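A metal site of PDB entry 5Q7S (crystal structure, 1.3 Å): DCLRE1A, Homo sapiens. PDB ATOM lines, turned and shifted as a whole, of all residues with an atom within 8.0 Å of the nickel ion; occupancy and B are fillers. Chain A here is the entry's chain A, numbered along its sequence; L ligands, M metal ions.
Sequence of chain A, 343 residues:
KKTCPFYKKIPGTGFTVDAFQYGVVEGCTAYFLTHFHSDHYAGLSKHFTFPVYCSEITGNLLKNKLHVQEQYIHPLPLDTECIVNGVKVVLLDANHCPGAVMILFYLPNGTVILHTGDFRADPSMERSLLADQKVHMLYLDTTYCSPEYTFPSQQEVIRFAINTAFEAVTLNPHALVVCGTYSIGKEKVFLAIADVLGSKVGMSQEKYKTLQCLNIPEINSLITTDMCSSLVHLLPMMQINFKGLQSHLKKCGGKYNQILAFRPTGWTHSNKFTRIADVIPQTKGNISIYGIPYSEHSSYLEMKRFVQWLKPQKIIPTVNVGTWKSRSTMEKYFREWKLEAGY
Four residues have an atom within 4 Å of the nickel ion: His 35, His 37, His 96 and Asp 118.
The nickel ion is bound by an oxygen (O3) of the ligand (2.0 Å), the side-chain carboxylate of Asp 118 (2.2 Å), an oxygen (O2) of the ligand (2.2 Å), a ring nitrogen (ND1) of His 37 (2.2 Å), a ring nitrogen (NE2) of His 96 (2.3 Å) and a ring nitrogen (NE2) of His 35 (2.3 Å).
NE2 of His 40 lies close to OD2 of Asp 118, 3.4 Å away. A ring nitrogen (NE2) of His 37 is in hydrogen-bond range of the side-chain sulfur (SG) of Cys 97 (3.8 Å). NE2 of His 37 sits at hydrogen-bond distance from O of Ile 184 (2.9 Å). The backbone carbonyl oxygen (O) of Glu 296 is in hydrogen-bond range of a ring nitrogen (ND1) of His 96. The side-chain hydroxyl of Thr 34 sits at hydrogen-bond distance from a ring nitrogen (ND1) of His 35, at 2.9 Å.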
ATOM      1  N   ASP A  18       6.743   9.261  14.551  1.00  0.00           N
ATOM      2  CA  ASP A  18       7.567  10.180  13.729  1.00  0.00           C
ATOM      3  C   ASP A  18       8.634   9.436  12.861  1.00  0.00           C
ATOM      4  O   ASP A  18       9.794   9.836  12.824  1.00  0.00           O
ATOM      5  CB  ASP A  18       8.148  11.297  14.579  1.00  0.00           C
ATOM      6  CG  ASP A  18       7.052  12.133  15.297  1.00  0.00           C
ATOM      7  OD1 ASP A  18       5.883  12.070  14.827  1.00  0.00           O
ATOM      8  OD2 ASP A  18       7.501  12.883  16.220  1.00  0.00           O
ATOM      9  N   THR A  34       3.389  13.236  15.641  1.00  0.00           N
ATOM     10  CA  THR A  34       3.205  14.205  16.727  1.00  0.00           C
ATOM     11  C   THR A  34       2.845  15.594  16.259  1.00  0.00           C
ATOM     12  O   THR A  34       2.042  16.277  16.921  1.00  0.00           O
ATOM     13  CB  THR A  34       4.370  14.223  17.702  1.00  0.00           C
ATOM     14  OG1 THR A  34       5.574  14.684  17.074  1.00  0.00           O
ATOM     15  CG2 THR A  34       4.672  12.883  18.394  1.00  0.00           C
ATOM     16  N   HIS A  35       3.521  16.061  15.173  1.00  0.00           N
ATOM     17  CA  HIS A  35       3.335  17.413  14.673  1.00  0.00           C
ATOM     18  C   HIS A  35       3.870  17.621  13.300  1.00  0.00           C
ATOM     19  O   HIS A  35       4.753  16.877  12.826  1.00  0.00           O
ATOM     20  CB  HIS A  35       3.926  18.420  15.705  1.00  0.00           C
ATOM     21  CG  HIS A  35       5.411  18.458  15.858  1.00  0.00           C
ATOM     22  ND1 HIS A  35       6.137  17.476  16.486  1.00  0.00           N
ATOM     23  CD2 HIS A  35       6.312  19.392  15.508  1.00  0.00           C
ATOM     24  CE1 HIS A  35       7.434  17.803  16.467  1.00  0.00           C
ATOM     25  NE2 HIS A  35       7.525  18.994  15.945  1.00  0.00           N
ATOM     26  N   PHE A  36       3.393  18.675  12.665  1.00  0.00           N
ATOM     27  CA  PHE A  36       3.818  19.053  11.277  1.00  0.00           C
ATOM     28  C   PHE A  36       5.158  19.883  11.206  1.00  0.00           C
ATOM     29  O   PHE A  36       5.108  21.076  10.834  1.00  0.00           O
ATOM     30  CB  PHE A  36       2.618  19.717  10.520  1.00  0.00           C
ATOM     31  CG  PHE A  36       2.777  19.758   8.991  1.00  0.00           C
ATOM     32  CD1 PHE A  36       2.530  18.616   8.243  1.00  0.00           C
ATOM     33  CD2 PHE A  36       3.105  20.942   8.342  1.00  0.00           C
ATOM     34  CE1 PHE A  36       2.689  18.663   6.844  1.00  0.00           C
ATOM     35  CE2 PHE A  36       3.225  20.983   6.929  1.00  0.00           C
ATOM     36  CZ  PHE A  36       3.036  19.861   6.198  1.00  0.00           C
ATOM     37  N   HIS A  37       6.285  19.360  11.608  1.00  0.00           N
ATOM     38  CA  HIS A  37       7.593  19.921  11.374  1.00  0.00           C
ATOM     39  C   HIS A  37       8.347  18.919  10.478  1.00  0.00           C
ATOM     40  O   HIS A  37       8.208  17.677  10.660  1.00  0.00           O
ATOM     41  CB  HIS A  37       8.356  20.214  12.703  1.00  0.00           C
ATOM     42  CG  HIS A  37       8.008  21.538  13.344  1.00  0.00           C
ATOM     43  ND1 HIS A  37       8.349  21.869  14.636  1.00  0.00           N
ATOM     44  CD2 HIS A  37       7.340  22.623  12.853  1.00  0.00           C
ATOM     45  CE1 HIS A  37       7.927  23.088  14.923  1.00  0.00           C
ATOM     46  NE2 HIS A  37       7.289  23.532  13.863  1.00  0.00           N
ATOM     47  N   SER A  38       9.220  19.454   9.586  1.00  0.00           N
ATOM     48  CA  SER A  38       9.785  18.614   8.511  1.00  0.00           C
ATOM     49  C   SER A  38      10.677  17.500   9.014  1.00  0.00           C
ATOM     50  O   SER A  38      10.649  16.451   8.364  1.00  0.00           O
ATOM     51  CB  SER A  38      10.468  19.434   7.396  1.00  0.00           C
ATOM     52  OG  SER A  38      11.537  20.133   7.935  1.00  0.00           O
ATOM     53  N   ASP A  39      11.460  17.688  10.075  1.00  0.00           N
ATOM     54  CA  ASP A  39      12.313  16.601  10.653  1.00  0.00           C
ATOM     55  C   ASP A  39      11.457  15.424  11.125  1.00  0.00           C
ATOM     56  O   ASP A  39      11.942  14.252  11.166  1.00  0.00           O
ATOM     57  CB  ASP A  39      13.263  17.088  11.756  1.00  0.00           C
ATOM     58  CG  ASP A  39      14.591  17.772  11.224  1.00  0.00           C
ATOM     59  OD1 ASP A  39      14.747  18.003  10.007  1.00  0.00           O
ATOM     60  OD2 ASP A  39      15.482  18.064  12.056  1.00  0.00           O
ATOM     61  N   HIS A  40      10.201  15.687  11.456  1.00  0.00           N
ATOM     62  CA  HIS A  40       9.321  14.622  11.959  1.00  0.00           C
ATOM     63  C   HIS A  40       8.451  13.983  10.911  1.00  0.00           C
ATOM     64  O   HIS A  40       8.287  12.753  10.974  1.00  0.00           O
ATOM     65  CB  HIS A  40       8.470  15.175  13.167  1.00  0.00           C
ATOM     66  CG  HIS A  40       9.327  15.628  14.296  1.00  0.00           C
ATOM     67  ND1 HIS A  40       9.457  14.925  15.476  1.00  0.00           N
ATOM     68  CD2 HIS A  40      10.129  16.703  14.433  1.00  0.00           C
ATOM     69  CE1 HIS A  40      10.326  15.529  16.272  1.00  0.00           C
ATOM     70  NE2 HIS A  40      10.760  16.619  15.641  1.00  0.00           N
ATOM     71  N   HIS A  96       3.636  23.213  21.883  1.00  0.00           N
ATOM     72  CA  HIS A  96       4.715  23.388  20.881  1.00  0.00           C
ATOM     73  C   HIS A  96       4.137  24.276  19.763  1.00  0.00           C
ATOM     74  O   HIS A  96       3.844  25.450  20.046  1.00  0.00           O
ATOM     75  CB  HIS A  96       5.270  21.999  20.441  1.00  0.00           C
ATOM     76  CG  HIS A  96       6.465  22.018  19.507  1.00  0.00           C
ATOM     77  ND1 HIS A  96       7.641  22.711  19.754  1.00  0.00           N
ATOM     78  CD2 HIS A  96       6.607  21.407  18.313  1.00  0.00           C
ATOM     79  CE1 HIS A  96       8.498  22.453  18.751  1.00  0.00           C
ATOM     80  NE2 HIS A  96       7.882  21.674  17.857  1.00  0.00           N
ATOM     81  N   CYS A  97       3.938  23.767  18.563  1.00  0.00           N
ATOM     82  CA  CYS A  97       3.313  24.554  17.452  1.00  0.00           C
ATOM     83  C   CYS A  97       1.856  24.087  17.316  1.00  0.00           C
ATOM     84  O   CYS A  97       1.490  23.087  17.970  1.00  0.00           O
ATOM     85  CB  CYS A  97       4.101  24.241  16.198  1.00  0.00           C
ATOM     86  SG  CYS A  97       4.087  22.497  15.605  1.00  0.00           S
ATOM     87  N   ALA A 100       0.390  20.207  17.642  1.00  0.00           N
ATOM     88  CA  ALA A 100       1.409  19.318  18.215  1.00  0.00           C
ATOM     89  C   ALA A 100       0.852  18.619  19.464  1.00  0.00           C
ATOM     90  O   ALA A 100       0.195  19.230  20.304  1.00  0.00           O
ATOM     91  CB  ALA A 100       2.676  20.123  18.605  1.00  0.00           C
ATOM     92  N   GLY A 117       6.762  13.919  22.090  1.00  0.00           N
ATOM     93  CA  GLY A 117       7.024  14.645  20.788  1.00  0.00           C
ATOM     94  C   GLY A 117       7.984  15.732  21.073  1.00  0.00           C
ATOM     95  O   GLY A 117       8.798  15.616  21.978  1.00  0.00           O
ATOM     96  N   ASP A 118       7.805  16.889  20.384  1.00  0.00           N
ATOM     97  CA  ASP A 118       8.415  18.175  20.767  1.00  0.00           C
ATOM     98  C   ASP A 118       7.430  18.903  21.712  1.00  0.00           C
ATOM     99  O   ASP A 118       6.198  18.935  21.460  1.00  0.00           O
ATOM    100  CB  ASP A 118       8.742  19.049  19.562  1.00  0.00           C
ATOM    101  CG  ASP A 118       9.983  18.621  18.740  1.00  0.00           C
ATOM    102  OD1 ASP A 118      10.771  17.844  19.246  1.00  0.00           O
ATOM    103  OD2 ASP A 118      10.048  19.210  17.664  1.00  0.00           O
ATOM    104  N   PHE A 119       7.945  19.441  22.792  1.00  0.00           N
ATOM    105  CA  PHE A 119       7.061  20.110  23.835  1.00  0.00           C
ATOM    106  C   PHE A 119       7.762  21.231  24.554  1.00  0.00           C
ATOM    107  O   PHE A 119       8.968  21.313  24.636  1.00  0.00           O
ATOM    108  CB  PHE A 119       6.366  19.127  24.824  1.00  0.00           C
ATOM    109  CG  PHE A 119       7.119  18.711  26.119  1.00  0.00           C
ATOM    110  CD1 PHE A 119       6.426  18.576  27.349  1.00  0.00           C
ATOM    111  CD2 PHE A 119       8.471  18.305  26.090  1.00  0.00           C
ATOM    112  CE1 PHE A 119       7.064  18.080  28.492  1.00  0.00           C
ATOM    113  CE2 PHE A 119       9.110  17.923  27.261  1.00  0.00           C
ATOM    114  CZ  PHE A 119       8.391  17.773  28.414  1.00  0.00           C
ATOM    115  N   ASP A 141      11.615  14.968  24.944  1.00  0.00           N
ATOM    116  CA  ASP A 141      12.239  16.081  24.165  1.00  0.00           C
ATOM    117  C   ASP A 141      13.237  16.752  25.086  1.00  0.00           C
ATOM    118  O   ASP A 141      12.872  17.574  25.876  1.00  0.00           O
ATOM    119  CB  ASP A 141      11.199  17.078  23.646  1.00  0.00           C
ATOM    120  CG  ASP A 141      11.772  18.345  23.097  1.00  0.00           C
ATOM    121  OD1 ASP A 141      12.981  18.335  22.752  1.00  0.00           O
ATOM    122  OD2 ASP A 141      10.961  19.286  22.920  1.00  0.00           O
ATOM    123  N   THR A 143      15.812  18.748  23.922  1.00  0.00           N
ATOM    124  CA  THR A 143      16.452  19.798  23.185  1.00  0.00           C
ATOM    125  C   THR A 143      17.344  20.678  24.014  1.00  0.00           C
ATOM    126  O   THR A 143      18.552  20.833  23.627  1.00  0.00           O
ATOM    127  CB  THR A 143      15.421  20.645  22.365  1.00  0.00           C
ATOM    128  OG1 THR A 143      14.737  19.852  21.423  1.00  0.00           O
ATOM    129  CG2 THR A 143      16.024  21.745  21.582  1.00  0.00           C
ATOM    130  N   SER A 183       8.465  27.741   9.163  1.00  0.00           N
ATOM    131  CA  SER A 183       7.703  26.549   9.464  1.00  0.00           C
ATOM    132  C   SER A 183       6.460  27.040  10.196  1.00  0.00           C
ATOM    133  O   SER A 183       6.254  28.250  10.445  1.00  0.00           O
ATOM    134  CB  SER A 183       8.501  25.604  10.385  1.00  0.00           C
ATOM    135  OG  SER A 183       8.770  26.178  11.635  1.00  0.00           O
ATOM    136  N   ILE A 184       5.624  26.123  10.571  1.00  0.00           N
ATOM    137  CA  ILE A 184       4.551  26.489  11.496  1.00  0.00           C
ATOM    138  C   ILE A 184       5.139  26.669  12.955  1.00  0.00           C
ATOM    139  O   ILE A 184       6.211  26.187  13.257  1.00  0.00           O
ATOM    140  CB  ILE A 184       3.355  25.555  11.455  1.00  0.00           C
ATOM    141  CG1 ILE A 184       3.719  24.171  11.960  1.00  0.00           C
ATOM    142  CG2 ILE A 184       2.676  25.611  10.080  1.00  0.00           C
ATOM    143  CD1 ILE A 184       2.489  23.371  12.358  1.00  0.00           C
ATOM    144  N   GLU A 296       9.631  27.475  21.489  1.00  0.00           N
ATOM    145  CA  GLU A 296       8.589  26.412  21.637  1.00  0.00           C
ATOM    146  C   GLU A 296       9.065  25.037  22.182  1.00  0.00           C
ATOM    147  O   GLU A 296       8.387  24.012  22.053  1.00  0.00           O
ATOM    148  CB  GLU A 296       7.689  26.280  20.361  1.00  0.00           C
ATOM    149  CG  GLU A 296       6.836  27.579  20.074  1.00  0.00           C
ATOM    150  CD  GLU A 296       5.874  27.487  18.919  1.00  0.00           C
ATOM    151  OE1 GLU A 296       6.095  26.725  17.958  1.00  0.00           O
ATOM    152  OE2 GLU A 296       4.938  28.388  18.927  1.00  0.00           O
ATOM    153  N   HIS A 297      10.258  25.091  22.835  1.00  0.00           N
ATOM    154  CA  HIS A 297      10.798  23.918  23.573  1.00  0.00           C
ATOM    155  C   HIS A 297      11.011  24.297  25.033  1.00  0.00           C
ATOM    156  O   HIS A 297      11.326  25.495  25.336  1.00  0.00           O
ATOM    157  CB  HIS A 297      12.149  23.446  22.988  1.00  0.00           C
ATOM    158  CG  HIS A 297      12.052  22.822  21.625  1.00  0.00           C
ATOM    159  ND1 HIS A 297      11.743  21.497  21.374  1.00  0.00           N
ATOM    160  CD2 HIS A 297      12.297  23.373  20.411  1.00  0.00           C
ATOM    161  CE1 HIS A 297      11.753  21.266  20.079  1.00  0.00           C
ATOM    162  NE2 HIS A 297      12.085  22.391  19.456  1.00  0.00           N
HETATM  163  C1  LIG L   1      12.146  21.803  14.800  1.00  0.00           C
HETATM  164  C2  LIG L   1      11.818  22.354  16.177  1.00  0.00           C
HETATM  165  C3  LIG L   1      11.766  20.336  14.623  1.00  0.00           C
HETATM  166  O1  LIG L   1      12.546  23.116  16.772  1.00  0.00           O
HETATM  167  O2  LIG L   1      10.764  22.095  16.711  1.00  0.00           O
HETATM  168  O3  LIG L   1      10.641  19.995  15.063  1.00  0.00           O
HETATM  169  O4  LIG L   1      12.580  19.660  13.955  1.00  0.00           O
HETATM  170 NI    NI M   1       9.173  20.610  16.275  1.00  0.00          NI
